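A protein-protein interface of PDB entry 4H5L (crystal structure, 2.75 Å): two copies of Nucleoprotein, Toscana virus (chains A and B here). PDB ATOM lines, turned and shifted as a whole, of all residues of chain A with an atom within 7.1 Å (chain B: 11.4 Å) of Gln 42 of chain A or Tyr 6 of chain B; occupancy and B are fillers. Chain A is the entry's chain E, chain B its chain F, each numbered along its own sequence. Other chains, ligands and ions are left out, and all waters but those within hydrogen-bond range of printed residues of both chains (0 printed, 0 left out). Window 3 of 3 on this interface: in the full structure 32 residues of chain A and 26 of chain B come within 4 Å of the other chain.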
ATOM      1  N   ASP A  36      25.157 -26.648  -0.067  1.00  0.00           N
ATOM      2  CA  ASP A  36      24.405 -27.904  -0.080  1.00  0.00           C
ATOM      3  C   ASP A  36      22.909 -27.588  -0.254  1.00  0.00           C
ATOM      4  O   ASP A  36      22.264 -27.151   0.703  1.00  0.00           O
ATOM      5  CB  ASP A  36      24.675 -28.756   1.181  1.00  0.00           C
ATOM      6  CG  ASP A  36      24.370 -30.245   1.046  1.00  0.00           C
ATOM      7  OD1 ASP A  36      24.471 -30.779  -0.089  1.00  0.00           O
ATOM      8  OD2 ASP A  36      24.093 -30.889   2.083  1.00  0.00           O
ATOM      9  N   PRO A  37      22.352 -27.749  -1.481  1.00  0.00           N
ATOM     10  CA  PRO A  37      20.931 -27.439  -1.695  1.00  0.00           C
ATOM     11  C   PRO A  37      20.041 -28.375  -0.900  1.00  0.00           C
ATOM     12  O   PRO A  37      18.992 -27.943  -0.448  1.00  0.00           O
ATOM     13  CB  PRO A  37      20.751 -27.623  -3.205  1.00  0.00           C
ATOM     14  CG  PRO A  37      22.129 -27.552  -3.768  1.00  0.00           C
ATOM     15  CD  PRO A  37      22.953 -28.239  -2.733  1.00  0.00           C
ATOM     16  N   LYS A  38      20.493 -29.623  -0.674  1.00  0.00           N
ATOM     17  CA  LYS A  38      19.771 -30.623   0.111  1.00  0.00           C
ATOM     18  C   LYS A  38      19.626 -30.158   1.554  1.00  0.00           C
ATOM     19  O   LYS A  38      18.542 -30.254   2.119  1.00  0.00           O
ATOM     20  CB  LYS A  38      20.500 -31.983   0.075  1.00  0.00           C
ATOM     21  CG  LYS A  38      20.533 -32.672  -1.283  1.00  0.00           C
ATOM     22  CD  LYS A  38      21.505 -33.849  -1.284  1.00  0.00           C
ATOM     23  CE  LYS A  38      21.476 -34.609  -2.591  1.00  0.00           C
ATOM     24  NZ  LYS A  38      22.592 -35.589  -2.700  1.00  0.00           N
ATOM     25  N   ARG A  39      20.720 -29.633   2.136  1.00  0.00           N
ATOM     26  CA  ARG A  39      20.781 -29.175   3.522  1.00  0.00           C
ATOM     27  C   ARG A  39      19.907 -27.951   3.761  1.00  0.00           C
ATOM     28  O   ARG A  39      19.240 -27.897   4.794  1.00  0.00           O
ATOM     29  CB  ARG A  39      22.235 -28.875   3.937  1.00  0.00           C
ATOM     30  CG  ARG A  39      22.454 -28.700   5.439  1.00  0.00           C
ATOM     31  CD  ARG A  39      22.604 -30.015   6.175  1.00  0.00           C
ATOM     32  NE  ARG A  39      22.645 -29.828   7.627  1.00  0.00           N
ATOM     33  CZ  ARG A  39      21.629 -30.077   8.449  1.00  0.00           C
ATOM     34  NH1 ARG A  39      20.475 -30.527   7.972  1.00  0.00           N
ATOM     35  NH2 ARG A  39      21.763 -29.890   9.755  1.00  0.00           N
ATOM     36  N   ILE A  40      19.896 -26.981   2.824  1.00  0.00           N
ATOM     37  CA  ILE A  40      19.119 -25.757   3.006  1.00  0.00           C
ATOM     38  C   ILE A  40      17.612 -26.017   2.756  1.00  0.00           C
ATOM     39  O   ILE A  40      16.794 -25.414   3.453  1.00  0.00           O
ATOM     40  CB  ILE A  40      19.672 -24.524   2.244  1.00  0.00           C
ATOM     41  CG1 ILE A  40      19.372 -24.523   0.742  1.00  0.00           C
ATOM     42  CG2 ILE A  40      21.155 -24.253   2.560  1.00  0.00           C
ATOM     43  CD1 ILE A  40      18.633 -23.268   0.360  1.00  0.00           C
ATOM     44  N   VAL A  41      17.248 -26.943   1.829  1.00  0.00           N
ATOM     45  CA  VAL A  41      15.852 -27.359   1.592  1.00  0.00           C
ATOM     46  C   VAL A  41      15.358 -28.034   2.890  1.00  0.00           C
ATOM     47  O   VAL A  41      14.240 -27.774   3.337  1.00  0.00           O
ATOM     48  CB  VAL A  41      15.708 -28.276   0.337  1.00  0.00           C
ATOM     49  CG1 VAL A  41      14.377 -29.025   0.323  1.00  0.00           C
ATOM     50  CG2 VAL A  41      15.868 -27.474  -0.954  1.00  0.00           C
ATOM     51  N   GLN A  42      16.238 -28.844   3.516  1.00  0.00           N
ATOM     52  CA  GLN A  42      15.999 -29.548   4.772  1.00  0.00           C
ATOM     53  C   GLN A  42      15.826 -28.552   5.927  1.00  0.00           C
ATOM     54  O   GLN A  42      14.807 -28.602   6.612  1.00  0.00           O
ATOM     55  CB  GLN A  42      17.153 -30.528   5.066  1.00  0.00           C
ATOM     56  CG  GLN A  42      16.989 -31.327   6.360  1.00  0.00           C
ATOM     57  CD  GLN A  42      18.091 -32.331   6.605  1.00  0.00           C
ATOM     58  OE1 GLN A  42      19.215 -32.225   6.091  1.00  0.00           O
ATOM     59  NE2 GLN A  42      17.794 -33.319   7.435  1.00  0.00           N
ATOM     60  N   LEU A  43      16.807 -27.642   6.119  1.00  0.00           N
ATOM     61  CA  LEU A  43      16.799 -26.649   7.195  1.00  0.00           C
ATOM     62  C   LEU A  43      15.641 -25.640   7.069  1.00  0.00           C
ATOM     63  O   LEU A  43      15.134 -25.209   8.101  1.00  0.00           O
ATOM     64  CB  LEU A  43      18.147 -25.922   7.310  1.00  0.00           C
ATOM     65  CG  LEU A  43      19.254 -26.681   8.074  1.00  0.00           C
ATOM     66  CD1 LEU A  43      20.626 -26.224   7.642  1.00  0.00           C
ATOM     67  CD2 LEU A  43      19.106 -26.530   9.592  1.00  0.00           C
ATOM     68  N   VAL A  44      15.185 -25.309   5.846  1.00  0.00           N
ATOM     69  CA  VAL A  44      14.020 -24.433   5.654  1.00  0.00           C
ATOM     70  C   VAL A  44      12.769 -25.176   6.164  1.00  0.00           C
ATOM     71  O   VAL A  44      12.023 -24.615   6.974  1.00  0.00           O
ATOM     72  CB  VAL A  44      13.872 -23.948   4.188  1.00  0.00           C
ATOM     73  CG1 VAL A  44      12.436 -23.570   3.868  1.00  0.00           C
ATOM     74  CG2 VAL A  44      14.803 -22.777   3.906  1.00  0.00           C
ATOM     75  N   LYS A  45      12.576 -26.450   5.730  1.00  0.00           N
ATOM     76  CA  LYS A  45      11.446 -27.272   6.154  1.00  0.00           C
ATOM     77  C   LYS A  45      11.477 -27.484   7.664  1.00  0.00           C
ATOM     78  O   LYS A  45      10.504 -27.152   8.330  1.00  0.00           O
ATOM     79  CB  LYS A  45      11.454 -28.610   5.429  1.00  0.00           C
ATOM     80  N   GLU A  46      12.623 -27.941   8.203  1.00  0.00           N
ATOM     81  CA  GLU A  46      12.823 -28.225   9.627  1.00  0.00           C
ATOM     82  C   GLU A  46      12.564 -27.001  10.496  1.00  0.00           C
ATOM     83  O   GLU A  46      11.736 -27.091  11.400  1.00  0.00           O
ATOM     84  CB  GLU A  46      14.232 -28.786   9.897  1.00  0.00           C
ATOM     85  CG  GLU A  46      14.379 -30.254   9.519  1.00  0.00           C
ATOM     86  CD  GLU A  46      15.724 -30.916   9.760  1.00  0.00           C
ATOM     87  OE1 GLU A  46      16.649 -30.248  10.277  1.00  0.00           O
ATOM     88  OE2 GLU A  46      15.850 -32.120   9.437  1.00  0.00           O
ATOM     89  N   ARG A  47      13.242 -25.863  10.213  1.00  0.00           N
ATOM     90  CA  ARG A  47      13.097 -24.617  10.977  1.00  0.00           C
ATOM     91  C   ARG A  47      11.708 -24.016  10.813  1.00  0.00           C
ATOM     92  O   ARG A  47      11.136 -23.550  11.800  1.00  0.00           O
ATOM     93  CB  ARG A  47      14.160 -23.582  10.590  1.00  0.00           C
ATOM     94  CG  ARG A  47      15.555 -23.899  11.124  1.00  0.00           C
ATOM     95  CD  ARG A  47      16.605 -22.986  10.523  1.00  0.00           C
ATOM     96  NE  ARG A  47      17.957 -23.452  10.829  1.00  0.00           N
ATOM     97  CZ  ARG A  47      19.070 -22.861  10.412  1.00  0.00           C
ATOM     98  NH1 ARG A  47      19.011 -21.762   9.672  1.00  0.00           N
ATOM     99  NH2 ARG A  47      20.251 -23.359  10.742  1.00  0.00           N
ATOM    100  N   GLY A  48      11.178 -24.062   9.587  1.00  0.00           N
ATOM    101  CA  GLY A  48       9.856 -23.547   9.252  1.00  0.00           C
ATOM    102  C   GLY A  48       8.719 -24.307   9.909  1.00  0.00           C
ATOM    103  O   GLY A  48       7.801 -23.686  10.454  1.00  0.00           O
ATOM    104  N   ILE A 107      21.515 -20.418   6.004  1.00  0.00           N
ATOM    105  CA  ILE A 107      20.529 -20.076   4.979  1.00  0.00           C
ATOM    106  C   ILE A 107      20.649 -18.590   4.598  1.00  0.00           C
ATOM    107  O   ILE A 107      20.765 -17.731   5.478  1.00  0.00           O
ATOM    108  CB  ILE A 107      19.079 -20.428   5.427  1.00  0.00           C
ATOM    109  CG1 ILE A 107      18.965 -21.911   5.894  1.00  0.00           C
ATOM    110  CG2 ILE A 107      18.074 -20.123   4.308  1.00  0.00           C
ATOM    111  CD1 ILE A 107      17.658 -22.282   6.597  1.00  0.00           C
ATOM    112  N   ALA A 115      18.178 -23.165  -4.431  1.00  0.00           N
ATOM    113  CA  ALA A 115      17.693 -24.506  -4.125  1.00  0.00           C
ATOM    114  C   ALA A 115      16.251 -24.719  -4.567  1.00  0.00           C
ATOM    115  O   ALA A 115      15.924 -25.819  -5.026  1.00  0.00           O
ATOM    116  CB  ALA A 115      17.825 -24.798  -2.642  1.00  0.00           C
ATOM    117  N   PHE A 116      15.389 -23.693  -4.425  1.00  0.00           N
ATOM    118  CA  PHE A 116      13.984 -23.785  -4.834  1.00  0.00           C
ATOM    119  C   PHE A 116      13.779 -23.113  -6.199  1.00  0.00           C
ATOM    120  O   PHE A 116      12.717 -22.541  -6.453  1.00  0.00           O
ATOM    121  CB  PHE A 116      13.073 -23.166  -3.766  1.00  0.00           C
ATOM    122  CG  PHE A 116      13.073 -23.898  -2.452  1.00  0.00           C
ATOM    123  CD1 PHE A 116      12.145 -24.894  -2.196  1.00  0.00           C
ATOM    124  CD2 PHE A 116      13.985 -23.571  -1.455  1.00  0.00           C
ATOM    125  CE1 PHE A 116      12.134 -25.563  -0.968  1.00  0.00           C
ATOM    126  CE2 PHE A 116      13.970 -24.235  -0.224  1.00  0.00           C
ATOM    127  CZ  PHE A 116      13.049 -25.231   0.011  1.00  0.00           C
ATOM    128  N   PHE A 214      22.514 -31.821  -7.587  1.00  0.00           N
ATOM    129  CA  PHE A 214      21.184 -31.809  -6.957  1.00  0.00           C
ATOM    130  C   PHE A 214      20.104 -32.263  -7.957  1.00  0.00           C
ATOM    131  O   PHE A 214      19.410 -33.240  -7.685  1.00  0.00           O
ATOM    132  CB  PHE A 214      20.854 -30.410  -6.389  1.00  0.00           C
ATOM    133  CG  PHE A 214      19.612 -30.282  -5.522  1.00  0.00           C
ATOM    134  CD1 PHE A 214      19.411 -31.124  -4.430  1.00  0.00           C
ATOM    135  CD2 PHE A 214      18.697 -29.256  -5.736  1.00  0.00           C
ATOM    136  CE1 PHE A 214      18.283 -30.979  -3.608  1.00  0.00           C
ATOM    137  CE2 PHE A 214      17.578 -29.106  -4.905  1.00  0.00           C
ATOM    138  CZ  PHE A 214      17.382 -29.967  -3.845  1.00  0.00           C
ATOM    139  N   PHE A 215      20.004 -31.591  -9.122  1.00  0.00           N
ATOM    140  CA  PHE A 215      19.048 -31.955 -10.165  1.00  0.00           C
ATOM    141  C   PHE A 215      19.737 -32.782 -11.235  1.00  0.00           C
ATOM    142  O   PHE A 215      20.824 -32.414 -11.686  1.00  0.00           O
ATOM    143  CB  PHE A 215      18.389 -30.709 -10.783  1.00  0.00           C
ATOM    144  CG  PHE A 215      17.549 -29.909  -9.814  1.00  0.00           C
ATOM    145  CD1 PHE A 215      16.388 -30.447  -9.262  1.00  0.00           C
ATOM    146  CD2 PHE A 215      17.912 -28.618  -9.458  1.00  0.00           C
ATOM    147  CE1 PHE A 215      15.614 -29.708  -8.363  1.00  0.00           C
ATOM    148  CE2 PHE A 215      17.135 -27.879  -8.562  1.00  0.00           C
ATOM    149  CZ  PHE A 215      15.989 -28.427  -8.025  1.00  0.00           C
ATOM    150  N   ASN B   5      13.272 -37.901  -2.074  1.00  0.00           N
ATOM    151  CA  ASN B   5      14.312 -37.135  -1.392  1.00  0.00           C
ATOM    152  C   ASN B   5      13.930 -35.622  -1.323  1.00  0.00           C
ATOM    153  O   ASN B   5      12.759 -35.272  -1.505  1.00  0.00           O
ATOM    154  CB  ASN B   5      15.670 -37.355  -2.108  1.00  0.00           C
ATOM    155  CG  ASN B   5      16.900 -37.346  -1.208  1.00  0.00           C
ATOM    156  OD1 ASN B   5      16.855 -37.702  -0.016  1.00  0.00           O
ATOM    157  ND2 ASN B   5      18.044 -36.972  -1.775  1.00  0.00           N
ATOM    158  N   TYR B   6      14.914 -34.745  -1.020  1.00  0.00           N
ATOM    159  CA  TYR B   6      14.736 -33.296  -0.943  1.00  0.00           C
ATOM    160  C   TYR B   6      14.678 -32.681  -2.341  1.00  0.00           C
ATOM    161  O   TYR B   6      14.092 -31.609  -2.504  1.00  0.00           O
ATOM    162  CB  TYR B   6      15.842 -32.645  -0.095  1.00  0.00           C
ATOM    163  CG  TYR B   6      15.768 -33.050   1.359  1.00  0.00           C
ATOM    164  CD1 TYR B   6      14.800 -32.514   2.203  1.00  0.00           C
ATOM    165  CD2 TYR B   6      16.641 -33.995   1.884  1.00  0.00           C
ATOM    166  CE1 TYR B   6      14.698 -32.913   3.534  1.00  0.00           C
ATOM    167  CE2 TYR B   6      16.555 -34.398   3.217  1.00  0.00           C
ATOM    168  CZ  TYR B   6      15.581 -33.853   4.039  1.00  0.00           C
ATOM    169  OH  TYR B   6      15.489 -34.230   5.358  1.00  0.00           O
ATOM    170  N   ARG B   7      15.237 -33.373  -3.353  1.00  0.00           N
ATOM    171  CA  ARG B   7      15.187 -32.936  -4.751  1.00  0.00           C
ATOM    172  C   ARG B   7      13.728 -32.950  -5.240  1.00  0.00           C
ATOM    173  O   ARG B   7      13.331 -32.103  -6.050  1.00  0.00           O
ATOM    174  CB  ARG B   7      16.069 -33.838  -5.622  1.00  0.00           C
ATOM    175  CG  ARG B   7      16.081 -33.480  -7.104  1.00  0.00           C
ATOM    176  CD  ARG B   7      16.406 -34.703  -7.930  1.00  0.00           C
ATOM    177  NE  ARG B   7      15.244 -35.175  -8.680  1.00  0.00           N
ATOM    178  CZ  ARG B   7      14.382 -36.086  -8.244  1.00  0.00           C
ATOM    179  NH1 ARG B   7      14.544 -36.647  -7.049  1.00  0.00           N
ATOM    180  NH2 ARG B   7      13.352 -36.448  -8.998  1.00  0.00           N
ATOM    181  N   ASP B   8      12.932 -33.901  -4.711  1.00  0.00           N
ATOM    182  CA  ASP B   8      11.511 -34.046  -5.015  1.00  0.00           C
ATOM    183  C   ASP B   8      10.718 -32.846  -4.474  1.00  0.00           C
ATOM    184  O   ASP B   8       9.871 -32.319  -5.198  1.00  0.00           O
ATOM    185  CB  ASP B   8      10.969 -35.376  -4.457  1.00  0.00           C
ATOM    186  CG  ASP B   8      11.432 -36.618  -5.216  1.00  0.00           C
ATOM    187  OD1 ASP B   8      11.695 -36.509  -6.449  1.00  0.00           O
ATOM    188  OD2 ASP B   8      11.464 -37.709  -4.602  1.00  0.00           O
ATOM    189  N   ILE B   9      11.033 -32.388  -3.233  1.00  0.00           N
ATOM    190  CA  ILE B   9      10.412 -31.227  -2.569  1.00  0.00           C
ATOM    191  C   ILE B   9      10.622 -29.965  -3.422  1.00  0.00           C
ATOM    192  O   ILE B   9       9.653 -29.263  -3.701  1.00  0.00           O
ATOM    193  CB  ILE B   9      10.954 -31.049  -1.125  1.00  0.00           C
ATOM    194  CG1 ILE B   9      10.475 -32.199  -0.219  1.00  0.00           C
ATOM    195  CG2 ILE B   9      10.565 -29.686  -0.536  1.00  0.00           C
ATOM    196  CD1 ILE B   9      11.313 -32.456   1.002  1.00  0.00           C
ATOM    197  N   ALA B  10      11.874 -29.702  -3.849  1.00  0.00           N
ATOM    198  CA  ALA B  10      12.234 -28.558  -4.687  1.00  0.00           C
ATOM    199  C   ALA B  10      11.529 -28.613  -6.050  1.00  0.00           C
ATOM    200  O   ALA B  10      11.055 -27.584  -6.529  1.00  0.00           O
ATOM    201  CB  ALA B  10      13.742 -28.497  -4.873  1.00  0.00           C
ATOM    202  N   LEU B  11      11.429 -29.814  -6.648  1.00  0.00           N
ATOM    203  CA  LEU B  11      10.765 -30.030  -7.936  1.00  0.00           C
ATOM    204  C   LEU B  11       9.250 -29.868  -7.837  1.00  0.00           C
ATOM    205  O   LEU B  11       8.616 -29.479  -8.822  1.00  0.00           O
ATOM    206  CB  LEU B  11      11.094 -31.427  -8.465  1.00  0.00           C
ATOM    207  CG  LEU B  11      12.346 -31.535  -9.311  1.00  0.00           C
ATOM    208  CD1 LEU B  11      12.806 -32.969  -9.401  1.00  0.00           C
ATOM    209  CD2 LEU B  11      12.093 -31.018 -10.693  1.00  0.00           C
ATOM    210  N   ALA B  12       8.676 -30.169  -6.643  1.00  0.00           N
ATOM    211  CA  ALA B  12       7.242 -30.056  -6.350  1.00  0.00           C
ATOM    212  C   ALA B  12       6.768 -28.601  -6.438  1.00  0.00           C
ATOM    213  O   ALA B  12       5.572 -28.360  -6.637  1.00  0.00           O
ATOM    214  CB  ALA B  12       6.937 -30.621  -4.975  1.00  0.00           C
ATOM    215  N   PHE B  13       7.715 -27.638  -6.330  1.00  0.00           N
ATOM    216  CA  PHE B  13       7.454 -26.205  -6.421  1.00  0.00           C
ATOM    217  C   PHE B  13       7.095 -25.769  -7.851  1.00  0.00           C
ATOM    218  O   PHE B  13       6.705 -24.616  -8.047  1.00  0.00           O
ATOM    219  CB  PHE B  13       8.634 -25.396  -5.873  1.00  0.00           C
ATOM    220  CG  PHE B  13       8.488 -25.145  -4.397  1.00  0.00           C
ATOM    221  CD1 PHE B  13       8.004 -23.932  -3.927  1.00  0.00           C
ATOM    222  CD2 PHE B  13       8.783 -26.147  -3.471  1.00  0.00           C
ATOM    223  CE1 PHE B  13       7.822 -23.722  -2.560  1.00  0.00           C
ATOM    224  CE2 PHE B  13       8.617 -25.927  -2.099  1.00  0.00           C
ATOM    225  CZ  PHE B  13       8.136 -24.719  -1.653  1.00  0.00           C
ATOM    226  N   LEU B  14       7.170 -26.696  -8.831  1.00  0.00           N
ATOM    227  CA  LEU B  14       6.766 -26.436 -10.211  1.00  0.00           C
ATOM    228  C   LEU B  14       5.242 -26.332 -10.311  1.00  0.00           C
ATOM    229  O   LEU B  14       4.728 -25.601 -11.159  1.00  0.00           O
ATOM    230  CB  LEU B  14       7.264 -27.549 -11.128  1.00  0.00           C
ATOM    231  CG  LEU B  14       8.154 -27.130 -12.293  1.00  0.00           C
ATOM    232  CD1 LEU B  14       8.720 -28.354 -12.979  1.00  0.00           C
ATOM    233  CD2 LEU B  14       7.403 -26.259 -13.296  1.00  0.00           C
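The side-chain hydroxyl of Tyr 6 of chain B lies within hydrogen-bond range of the side-chain amide nitrogen of Gln 42 of chain A (3.2 Å).
The side-chain amide oxygen (OE1) of Gln 42 of chain A lies within hydrogen-bond range of the guanidinium group (NH1) of Arg 39 of chain A.
The side-chain carboxylate of Asp 8 of chain B is in salt-bridge range of the guanidinium group of Arg 7 of chain B, at 2.9 Å.
The side-chain amide nitrogen (NE2) of Gln 42 of chain A lies within hydrogen-bond range of the side-chain carboxylate (OE2) of Glu 46 of chain A, 3.0 Å away.
Among the printed residues, pairs that only touch across the chains: Val 41 of chain A with Tyr 6 of chain B (3.8 Å), Val 41 of chain A with Ile 9 of chain B (3.96 Å), Ala 115 of chain A with Ala 10 of chain B (3.5 Å), Phe 116 of chain A with Phe 13 of chain B (3.7 Å), Phe 214 of chain A with Tyr 6 of chain B (3.9 Å), Phe 214 of chain A with Arg 7 of chain B (3.4 Å), Phe 214 of chain A with Ala 10 of chain B (3.9 Å), Phe 215 of chain A with Arg 7 of chain B (3.7 Å), Phe 215 of chain A with Ala 10 of chain B (3.9 Å) and Phe 215 of chain A with Leu 11 of chain B (3.9 Å).
Asp 36 of chain A touches none of the printed residues of chain B.
Lys 38 of chain A touches none of the printed residues of chain B.
Val 41 of chain A touches just these residues of chain B: Tyr 6 (3.8 Å) and Ile 9 (3.96 Å).
Of the printed residues of chain B, Gln 42 of chain A touches Tyr 6 (3.2 Å).
No residue of chain B comes within 4 Å of Leu 43 of chain A.
No residue of chain B comes within 4 Å of Val 44 of chain A.
No residue of chain B comes within 4 Å of Lys 45 of chain A.
Of the printed residues of chain B, Ala 115 of chain A touches Ala 10 (3.5 Å).
Of the printed residues of chain B, Phe 214 of chain A touches Tyr 6 (3.9 Å), Arg 7 (3.4 Å) and Ala 10 (3.9 Å).
Of the printed residues of chain A, Tyr 6 of chain B touches Val 41 (3.8 Å), Gln 42 (3.2 Å) and Phe 214 (3.9 Å).
Printed residues of chain A within 4 Å of Ile 9 of chain B: Val 41 (3.96 Å).
Of the printed residues of chain A, Ala 10 of chain B touches Ala 115, Phe 214 and Phe 215.
Printed residues of chain A within 4 Å of Phe 13 of chain B: Phe 116.
The nearest residue of chain B that does not touch Gln 42 of chain A is Ile 9 of chain B (6.6 Å).
The nearest printed residue of chain A that does not touch Tyr 6 of chain B is Lys 38 of chain A (4.01 Å).
The nearest printed residue of chain A that does not touch Ile 9 of chain B is Phe 116 of chain A (4.4 Å).
Of the 18 printed residues of chain A, 6 touch a printed residue of chain B.
Printed residues of chain A that touch a printed residue of chain B: Val 41, Gln 42, Ala 115, Phe 116, Phe 214 and Phe 215.
Along chain A the printed residues that touch a printed residue of chain B span positions 41 to 215.
Along chain B the printed residues that touch a printed residue of chain A span positions 6 to 13.
Among the printed residues, 11 pairs touch across the chains.
No position is printed for both chains.
Of the 11 pairs that touch across the chains among the printed residues, none has its exchanged pair printed and touching as well.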
